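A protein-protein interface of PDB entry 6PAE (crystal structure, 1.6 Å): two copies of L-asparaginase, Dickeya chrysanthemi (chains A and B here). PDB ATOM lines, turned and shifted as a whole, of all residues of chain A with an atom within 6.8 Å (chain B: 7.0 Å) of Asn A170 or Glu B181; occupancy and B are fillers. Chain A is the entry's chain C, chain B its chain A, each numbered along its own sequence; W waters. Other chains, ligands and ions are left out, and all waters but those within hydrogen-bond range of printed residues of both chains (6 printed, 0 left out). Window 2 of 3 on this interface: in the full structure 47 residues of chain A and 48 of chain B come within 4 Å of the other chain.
Asn A170 touches just these residues of chain B: Glu B181 (3.8 Å), Thr B279 (3.5 Å), Asn B281 (3.2 Å) and Gly B282 (3.6 Å).
Printed residues of chain A within 4 Å of Gly B251: Lys A168 (3.8 Å).
Of the printed residues of chain A, Thr B279 touches Lys A168 (3.1 Å), Thr A169 (3.2 Å), Asn A170 (3.5 Å) and Ala A171 (3.3 Å).
Of the printed residues of chain A, Gly B280 touches Thr A169.
Of the printed residues of chain A, Asn B281 touches Thr A169, Asn A170 and Ala A171.
Of the printed residues of chain A, Ile B283 touches Ala A171 and Ser A172.
Of the 13 printed residues of chain A, 5 touch a printed residue of chain B.
Printed residues of chain A that touch a printed residue of chain B: Lys A168, Thr A169, Asn A170, Ala A171 and Ser A172.
Printed residues of chain B that touch a printed residue of chain A: Glu B181, Gly B251, Ala B252, Thr B279, Gly B280, Asn B281, Gly B282 and Ile B283.
Along chain B the printed residues that touch a printed residue of chain A span positions 181 to 283.
Among the printed residues, pairs that only touch across the chains: Lys A168 with Gly B251, Lys A168 with Thr B279, Thr A169 with Gly B280, Asn A170 with Glu B181, Asn A170 with Thr B279, Asn A170 with Asn B281, Asn A170 with Gly B282, Ala A171 with Ala B252, Ala A171 with Ile B283 and Ser A172 with Ala B252.
OG1 of Thr B279 lies within hydrogen-bond range of N of Ala A171, at 3.3 Å.
The side-chain amide nitrogen (ND2) of Asn B281 sits at hydrogen-bond distance from the backbone carbonyl oxygen (O) of Thr A169, at 2.8 Å.
N of Ala A171 lies within hydrogen-bond range of O of Asn B281 (3.0 Å).
O of Ile B283 is in hydrogen-bond range of OG of Ser A172 (2.7 Å).
The backbone carbonyl oxygen (O) of Thr A169 sits close to the backbone carbonyl oxygen (O) of Thr B279 (3.2 Å).
Water W5 bridges OE2 of Glu B181 (2.7 Å) and ND2 of Asn A170 (2.9 Å).
Water W6 lies within hydrogen-bond range of OG1 of Thr A167, O of Thr B279 and O of Lys A168.
Water W1 bridges the side-chain hydroxyl of Thr A169 and the side-chain amide nitrogen of Asn B281.
Water W3 bridges the side-chain amide oxygen of Asn A170 (2.8 Å) and the backbone NH of Ile B283 (2.9 Å).
Water W4 lies within hydrogen-bond range of OE1 of Glu B181 (2.8 Å) and ND2 of Asn A170 (3.1 Å).
Water W2 lies within hydrogen-bond range of OE2 of Glu B181 (2.9 Å) and NH2 of Arg A178 (3.3 Å).
1 position is printed for both chains.
Of the 15 pairs that touch across the chains among the printed residues, none has its exchanged pair printed and touching as well.
ND2 of Asn B180 is in hydrogen-bond range of OD1 of Asn B281 (3.0 Å).
The side-chain hydroxyl (OG1) of Thr B277 sits at hydrogen-bond distance from the side-chain hydroxyl (OG1) of Thr B279, 2.8 Å away.
The side-chain hydroxyl of Thr B279 lies within hydrogen-bond range of the backbone carbonyl oxygen of Asn B281, at 3.3 Å.
The side-chain sulfur (SD) of Met A121 sits at hydrogen-bond distance from the side-chain amino group (NZ) of Lys A168 (3.5 Å).
The backbone NH (N) of Ser A172 sits at hydrogen-bond distance from the side-chain amide oxygen (OD1) of Asn A170.
The backbone carbonyl oxygen (O) of Asn A170 is in hydrogen-bond range of the side-chain hydroxyl (OG1) of Thr A176, 2.6 Å away.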
ATOM      1  N   MET A 121      20.683 -33.684 -12.331  1.00  0.00           N
ATOM      2  CA  MET A 121      19.846 -32.842 -13.186  1.00  0.00           C
ATOM      3  C   MET A 121      20.365 -32.636 -14.626  1.00  0.00           C
ATOM      4  O   MET A 121      19.575 -32.314 -15.524  1.00  0.00           O
ATOM      5  CB  MET A 121      19.618 -31.536 -12.452  1.00  0.00           C
ATOM      6  CG  MET A 121      18.650 -31.652 -11.317  1.00  0.00           C
ATOM      7  SD  MET A 121      16.946 -31.954 -11.794  1.00  0.00           S
ATOM      8  CE  MET A 121      16.513 -30.383 -12.584  1.00  0.00           C
ATOM      9  N   THR A 167      12.031 -32.612  -1.627  1.00  0.00           N
ATOM     10  CA  THR A 167      11.192 -32.622  -2.831  1.00  0.00           C
ATOM     11  C   THR A 167      11.926 -31.839  -3.936  1.00  0.00           C
ATOM     12  O   THR A 167      12.745 -30.935  -3.687  1.00  0.00           O
ATOM     13  CB  THR A 167       9.800 -32.026  -2.520  1.00  0.00           C
ATOM     14  OG1 THR A 167       9.048 -31.973  -3.746  1.00  0.00           O
ATOM     15  CG2 THR A 167       9.912 -30.615  -1.933  1.00  0.00           C
ATOM     16  N   LYS A 168      11.606 -32.193  -5.170  1.00  0.00           N
ATOM     17  CA  LYS A 168      12.084 -31.503  -6.382  1.00  0.00           C
ATOM     18  C   LYS A 168      11.246 -30.228  -6.463  1.00  0.00           C
ATOM     19  O   LYS A 168      10.048 -30.262  -6.681  1.00  0.00           O
ATOM     20  CB  LYS A 168      11.919 -32.391  -7.569  1.00  0.00           C
ATOM     21  CG  LYS A 168      12.590 -31.751  -8.807  1.00  0.00           C
ATOM     22  CD  LYS A 168      12.697 -32.677  -9.962  1.00  0.00           C
ATOM     23  CE  LYS A 168      13.282 -31.978 -11.146  1.00  0.00           C
ATOM     24  NZ  LYS A 168      13.630 -32.873 -12.304  1.00  0.00           N
ATOM     25  N   THR A 169      11.874 -29.082  -6.172  1.00  0.00           N
ATOM     26  CA  THR A 169      11.101 -27.804  -6.112  1.00  0.00           C
ATOM     27  C   THR A 169      11.226 -26.954  -7.366  1.00  0.00           C
ATOM     28  O   THR A 169      10.411 -26.009  -7.536  1.00  0.00           O
ATOM     29  CB  THR A 169      11.584 -26.888  -4.949  1.00  0.00           C
ATOM     30  OG1 THR A 169      12.893 -26.365  -5.196  1.00  0.00           O
ATOM     31  CG2 THR A 169      11.552 -27.580  -3.561  1.00  0.00           C
ATOM     32  N   ASN A 170      12.122 -27.299  -8.295  1.00  0.00           N
ATOM     33  CA  ASN A 170      12.309 -26.558  -9.530  1.00  0.00           C
ATOM     34  C   ASN A 170      12.395 -27.575 -10.696  1.00  0.00           C
ATOM     35  O   ASN A 170      13.031 -28.637 -10.584  1.00  0.00           O
ATOM     36  CB  ASN A 170      13.598 -25.741  -9.431  1.00  0.00           C
ATOM     37  CG  ASN A 170      13.763 -24.719 -10.536  1.00  0.00           C
ATOM     38  OD1 ASN A 170      13.900 -25.090 -11.725  1.00  0.00           O
ATOM     39  ND2 ASN A 170      13.751 -23.421 -10.184  1.00  0.00           N
ATOM     40  N   ALA A 171      11.786 -27.207 -11.823  1.00  0.00           N
ATOM     41  CA  ALA A 171      11.720 -28.037 -12.968  1.00  0.00           C
ATOM     42  C   ALA A 171      13.146 -28.466 -13.403  1.00  0.00           C
ATOM     43  O   ALA A 171      13.318 -29.564 -13.864  1.00  0.00           O
ATOM     44  CB  ALA A 171      11.014 -27.306 -14.125  1.00  0.00           C
ATOM     45  N   SER A 172      14.107 -27.541 -13.288  1.00  0.00           N
ATOM     46  CA  SER A 172      15.293 -27.548 -14.174  1.00  0.00           C
ATOM     47  C   SER A 172      16.630 -27.172 -13.560  1.00  0.00           C
ATOM     48  O   SER A 172      17.619 -27.334 -14.271  1.00  0.00           O
ATOM     49  CB  SER A 172      15.080 -26.655 -15.396  1.00  0.00           C
ATOM     50  OG  SER A 172      14.002 -27.193 -16.184  1.00  0.00           O
ATOM     51  N   THR A 173      16.695 -26.734 -12.293  1.00  0.00           N
ATOM     52  CA  THR A 173      17.999 -26.267 -11.756  1.00  0.00           C
ATOM     53  C   THR A 173      18.738 -27.362 -10.966  1.00  0.00           C
ATOM     54  O   THR A 173      18.130 -28.336 -10.479  1.00  0.00           O
ATOM     55  CB  THR A 173      17.755 -25.097 -10.837  1.00  0.00           C
ATOM     56  OG1 THR A 173      16.747 -25.487  -9.901  1.00  0.00           O
ATOM     57  CG2 THR A 173      17.288 -23.905 -11.596  1.00  0.00           C
ATOM     58  N   LEU A 174      20.061 -27.184 -10.842  1.00  0.00           N
ATOM     59  CA  LEU A 174      20.854 -28.121 -10.063  1.00  0.00           C
ATOM     60  C   LEU A 174      20.467 -28.190  -8.613  1.00  0.00           C
ATOM     61  O   LEU A 174      20.658 -29.271  -7.994  1.00  0.00           O
ATOM     62  CB  LEU A 174      22.324 -27.764 -10.143  1.00  0.00           C
ATOM     63  CG  LEU A 174      23.042 -27.929 -11.475  1.00  0.00           C
ATOM     64  CD1 LEU A 174      24.571 -27.728 -11.334  1.00  0.00           C
ATOM     65  CD2 LEU A 174      22.714 -29.290 -12.046  1.00  0.00           C
ATOM     66  N   ASP A 175      19.999 -27.039  -8.079  1.00  0.00           N
ATOM     67  CA  ASP A 175      19.730 -26.883  -6.655  1.00  0.00           C
ATOM     68  C   ASP A 175      18.270 -27.100  -6.325  1.00  0.00           C
ATOM     69  O   ASP A 175      17.798 -26.735  -5.232  1.00  0.00           O
ATOM     70  CB  ASP A 175      20.188 -25.521  -6.184  1.00  0.00           C
ATOM     71  CG  ASP A 175      19.703 -24.402  -7.026  1.00  0.00           C
ATOM     72  OD1 ASP A 175      20.086 -24.279  -8.199  1.00  0.00           O
ATOM     73  OD2 ASP A 175      18.926 -23.600  -6.494  1.00  0.00           O
ATOM     74  N   THR A 176      17.572 -27.804  -7.225  1.00  0.00           N
ATOM     75  CA  THR A 176      16.153 -28.063  -7.134  1.00  0.00           C
ATOM     76  C   THR A 176      15.699 -28.764  -5.842  1.00  0.00           C
ATOM     77  O   THR A 176      14.600 -28.488  -5.341  1.00  0.00           O
ATOM     78  CB  THR A 176      15.710 -28.840  -8.343  1.00  0.00           C
ATOM     79  OG1 THR A 176      14.290 -28.999  -8.306  1.00  0.00           O
ATOM     80  CG2 THR A 176      16.419 -30.193  -8.583  1.00  0.00           C
ATOM     81  N   PHE A 177      16.486 -29.716  -5.277  1.00  0.00           N
ATOM     82  CA  PHE A 177      16.039 -30.445  -4.103  1.00  0.00           C
ATOM     83  C   PHE A 177      16.252 -29.634  -2.873  1.00  0.00           C
ATOM     84  O   PHE A 177      17.376 -29.301  -2.483  1.00  0.00           O
ATOM     85  CB  PHE A 177      16.747 -31.779  -4.001  1.00  0.00           C
ATOM     86  CG  PHE A 177      16.245 -32.759  -5.033  1.00  0.00           C
ATOM     87  CD1 PHE A 177      15.083 -33.470  -4.806  1.00  0.00           C
ATOM     88  CD2 PHE A 177      16.898 -32.879  -6.226  1.00  0.00           C
ATOM     89  CE1 PHE A 177      14.580 -34.363  -5.749  1.00  0.00           C
ATOM     90  CE2 PHE A 177      16.366 -33.744  -7.201  1.00  0.00           C
ATOM     91  CZ  PHE A 177      15.161 -34.420  -6.980  1.00  0.00           C
ATOM     92  N   ARG A 178      15.136 -29.238  -2.258  1.00  0.00           N
ATOM     93  CA  ARG A 178      15.123 -28.416  -1.054  1.00  0.00           C
ATOM     94  C   ARG A 178      13.993 -28.918  -0.152  1.00  0.00           C
ATOM     95  O   ARG A 178      13.008 -29.520  -0.641  1.00  0.00           O
ATOM     96  CB  ARG A 178      14.792 -26.941  -1.365  1.00  0.00           C
ATOM     97  CG  ARG A 178      15.479 -26.305  -2.563  1.00  0.00           C
ATOM     98  CD  ARG A 178      16.543 -25.393  -2.141  1.00  0.00           C
ATOM     99  NE  ARG A 178      17.068 -24.526  -3.230  1.00  0.00           N
ATOM    100  CZ  ARG A 178      16.721 -23.276  -3.538  1.00  0.00           C
ATOM    101  NH1 ARG A 178      15.690 -22.617  -3.006  1.00  0.00           N
ATOM    102  NH2 ARG A 178      17.388 -22.706  -4.533  1.00  0.00           N
ATOM    103  N   TYR B 165       4.180 -13.808 -11.033  1.00  0.00           N
ATOM    104  CA  TYR B 165       5.145 -14.655 -10.337  1.00  0.00           C
ATOM    105  C   TYR B 165       4.720 -15.175  -8.972  1.00  0.00           C
ATOM    106  O   TYR B 165       5.157 -16.247  -8.546  1.00  0.00           O
ATOM    107  CB  TYR B 165       6.470 -13.911 -10.259  1.00  0.00           C
ATOM    108  CG  TYR B 165       7.120 -13.483 -11.540  1.00  0.00           C
ATOM    109  CD1 TYR B 165       7.096 -14.278 -12.655  1.00  0.00           C
ATOM    110  CD2 TYR B 165       7.772 -12.249 -11.658  1.00  0.00           C
ATOM    111  CE1 TYR B 165       7.714 -13.900 -13.802  1.00  0.00           C
ATOM    112  CE2 TYR B 165       8.440 -11.893 -12.809  1.00  0.00           C
ATOM    113  CZ  TYR B 165       8.367 -12.682 -13.900  1.00  0.00           C
ATOM    114  OH  TYR B 165       8.958 -12.343 -15.095  1.00  0.00           O
ATOM    115  N   ARG B 178       5.399 -15.963  -1.910  1.00  0.00           N
ATOM    116  CA  ARG B 178       6.832 -15.866  -2.329  1.00  0.00           C
ATOM    117  C   ARG B 178       6.916 -16.130  -3.819  1.00  0.00           C
ATOM    118  O   ARG B 178       6.037 -16.781  -4.443  1.00  0.00           O
ATOM    119  CB  ARG B 178       7.701 -16.852  -1.576  1.00  0.00           C
ATOM    120  CG  ARG B 178       7.755 -16.524  -0.094  1.00  0.00           C
ATOM    121  CD  ARG B 178       8.490 -17.594   0.614  1.00  0.00           C
ATOM    122  NE  ARG B 178       8.587 -17.373   2.060  1.00  0.00           N
ATOM    123  CZ  ARG B 178       9.369 -18.151   2.814  1.00  0.00           C
ATOM    124  NH1 ARG B 178      10.095 -19.157   2.274  1.00  0.00           N
ATOM    125  NH2 ARG B 178       9.379 -18.006   4.110  1.00  0.00           N
ATOM    126  N   ALA B 179       7.936 -15.582  -4.437  1.00  0.00           N
ATOM    127  CA  ALA B 179       8.314 -15.842  -5.817  1.00  0.00           C
ATOM    128  C   ALA B 179       9.778 -16.223  -5.775  1.00  0.00           C
ATOM    129  O   ALA B 179      10.675 -15.349  -5.789  1.00  0.00           O
ATOM    130  CB  ALA B 179       8.055 -14.617  -6.708  1.00  0.00           C
ATOM    131  N   ASN B 180      10.048 -17.515  -5.602  1.00  0.00           N
ATOM    132  CA  ASN B 180      11.387 -17.914  -5.189  1.00  0.00           C
ATOM    133  C   ASN B 180      12.499 -17.472  -6.174  1.00  0.00           C
ATOM    134  O   ASN B 180      13.611 -17.011  -5.749  1.00  0.00           O
ATOM    135  CB  ASN B 180      11.494 -19.387  -4.903  1.00  0.00           C
ATOM    136  CG  ASN B 180      10.609 -19.816  -3.764  1.00  0.00           C
ATOM    137  OD1 ASN B 180      10.666 -19.263  -2.639  1.00  0.00           O
ATOM    138  ND2 ASN B 180       9.745 -20.773  -4.047  1.00  0.00           N
ATOM    139  N   GLU B 181      12.223 -17.571  -7.463  1.00  0.00           N
ATOM    140  CA  GLU B 181      13.180 -17.263  -8.493  1.00  0.00           C
ATOM    141  C   GLU B 181      13.077 -15.795  -8.972  1.00  0.00           C
ATOM    142  O   GLU B 181      14.057 -15.300  -9.490  1.00  0.00           O
ATOM    143  CB  GLU B 181      13.044 -18.194  -9.682  1.00  0.00           C
ATOM    144  CG  GLU B 181      13.377 -19.639  -9.296  1.00  0.00           C
ATOM    145  CD  GLU B 181      14.872 -19.879  -9.181  1.00  0.00           C
ATOM    146  OE1 GLU B 181      15.613 -19.571 -10.181  1.00  0.00           O
ATOM    147  OE2 GLU B 181      15.274 -20.436  -8.128  1.00  0.00           O
ATOM    148  N   GLU B 182      11.918 -15.125  -8.790  1.00  0.00           N
ATOM    149  CA  GLU B 182      11.721 -13.802  -9.332  1.00  0.00           C
ATOM    150  C   GLU B 182      11.629 -12.675  -8.288  1.00  0.00           C
ATOM    151  O   GLU B 182      11.680 -11.505  -8.624  1.00  0.00           O
ATOM    152  CB  GLU B 182      10.436 -13.778 -10.159  1.00  0.00           C
ATOM    153  CG  GLU B 182      10.362 -14.861 -11.212  1.00  0.00           C
ATOM    154  CD  GLU B 182       9.601 -16.111 -10.743  1.00  0.00           C
ATOM    155  OE1 GLU B 182       9.365 -16.370  -9.527  1.00  0.00           O
ATOM    156  OE2 GLU B 182       9.318 -16.955 -11.652  1.00  0.00           O
ATOM    157  N   GLY B 183      11.597 -13.039  -7.030  1.00  0.00           N
ATOM    158  CA  GLY B 183      11.455 -12.091  -5.930  1.00  0.00           C
ATOM    159  C   GLY B 183      10.217 -11.237  -6.013  1.00  0.00           C
ATOM    160  O   GLY B 183       9.235 -11.536  -6.691  1.00  0.00           O
ATOM    161  N   GLY B 251       8.790 -33.177 -12.518  1.00  0.00           N
ATOM    162  CA  GLY B 251       9.966 -32.507 -13.042  1.00  0.00           C
ATOM    163  C   GLY B 251       9.628 -31.444 -14.096  1.00  0.00           C
ATOM    164  O   GLY B 251       8.666 -30.661 -13.925  1.00  0.00           O
ATOM    165  N   ALA B 252      10.346 -31.484 -15.206  1.00  0.00           N
ATOM    166  CA  ALA B 252      10.240 -30.423 -16.224  1.00  0.00           C
ATOM    167  C   ALA B 252       9.176 -30.825 -17.248  1.00  0.00           C
ATOM    168  O   ALA B 252       9.494 -31.010 -18.451  1.00  0.00           O
ATOM    169  CB  ALA B 252      11.564 -30.189 -16.913  1.00  0.00           C
ATOM    170  N   THR B 277       4.598 -27.908 -14.385  1.00  0.00           N
ATOM    171  CA  THR B 277       5.325 -28.705 -13.430  1.00  0.00           C
ATOM    172  C   THR B 277       4.575 -28.628 -12.084  1.00  0.00           C
ATOM    173  O   THR B 277       4.097 -27.540 -11.694  1.00  0.00           O
ATOM    174  CB  THR B 277       6.780 -28.175 -13.318  1.00  0.00           C
ATOM    175  OG1 THR B 277       7.493 -28.968 -12.365  1.00  0.00           O
ATOM    176  CG2 THR B 277       6.854 -26.728 -12.920  1.00  0.00           C
ATOM    177  N   THR B 279       6.453 -29.008  -9.426  1.00  0.00           N
ATOM    178  CA  THR B 279       7.589 -28.854  -8.498  1.00  0.00           C
ATOM    179  C   THR B 279       7.474 -27.579  -7.662  1.00  0.00           C
ATOM    180  O   THR B 279       7.850 -27.537  -6.478  1.00  0.00           O
ATOM    181  CB  THR B 279       8.934 -28.810  -9.239  1.00  0.00           C
ATOM    182  OG1 THR B 279       8.896 -27.759 -10.229  1.00  0.00           O
ATOM    183  CG2 THR B 279       9.211 -30.168  -9.864  1.00  0.00           C
ATOM    184  N   GLY B 280       6.882 -26.563  -8.245  1.00  0.00           N
ATOM    185  CA  GLY B 280       6.683 -25.249  -7.605  1.00  0.00           C
ATOM    186  C   GLY B 280       7.366 -24.078  -8.305  1.00  0.00           C
ATOM    187  O   GLY B 280       6.948 -22.921  -8.141  1.00  0.00           O
ATOM    188  N   ASN B 281       8.397 -24.331  -9.095  1.00  0.00           N
ATOM    189  CA  ASN B 281       9.224 -23.245  -9.624  1.00  0.00           C
ATOM    190  C   ASN B 281       9.870 -23.683 -10.944  1.00  0.00           C
ATOM    191  O   ASN B 281      10.131 -24.864 -11.112  1.00  0.00           O
ATOM    192  CB  ASN B 281      10.395 -22.874  -8.611  1.00  0.00           C
ATOM    193  CG  ASN B 281       9.914 -22.569  -7.194  1.00  0.00           C
ATOM    194  OD1 ASN B 281       9.647 -21.456  -6.917  1.00  0.00           O
ATOM    195  ND2 ASN B 281       9.677 -23.632  -6.333  1.00  0.00           N
ATOM    196  N   GLY B 282      10.288 -22.691 -11.727  1.00  0.00           N
ATOM    197  CA  GLY B 282      11.256 -22.875 -12.770  1.00  0.00           C
ATOM    198  C   GLY B 282      10.667 -23.147 -14.135  1.00  0.00           C
ATOM    199  O   GLY B 282       9.476 -23.062 -14.371  1.00  0.00           O
ATOM    200  N   ILE B 283      11.558 -23.449 -15.031  1.00  0.00           N
ATOM    201  CA  ILE B 283      11.234 -23.448 -16.482  1.00  0.00           C
ATOM    202  C   ILE B 283      10.970 -24.873 -16.964  1.00  0.00           C
ATOM    203  O   ILE B 283      11.770 -25.810 -16.790  1.00  0.00           O
ATOM    204  CB  ILE B 283      12.413 -22.927 -17.300  1.00  0.00           C
ATOM    205  CG1 ILE B 283      12.729 -21.464 -16.983  1.00  0.00           C
ATOM    206  CG2 ILE B 283      12.189 -23.176 -18.774  1.00  0.00           C
ATOM    207  CD1 ILE B 283      11.779 -20.461 -17.460  1.00  0.00           C
HETATM  208  O   HOH W   1      12.841 -23.587  -5.034  1.00  0.00           O
HETATM  209  O   HOH W   2      16.989 -19.725  -5.962  1.00  0.00           O
HETATM  210  O   HOH W   3      14.286 -23.428 -13.954  1.00  0.00           O
HETATM  211  O   HOH W   4      14.371 -21.108 -12.219  1.00  0.00           O
HETATM  212  O   HOH W   5      13.867 -22.643  -7.343  1.00  0.00           O
HETATM  213  O   HOH W   6       7.664 -29.782  -4.675  1.00  0.00           O
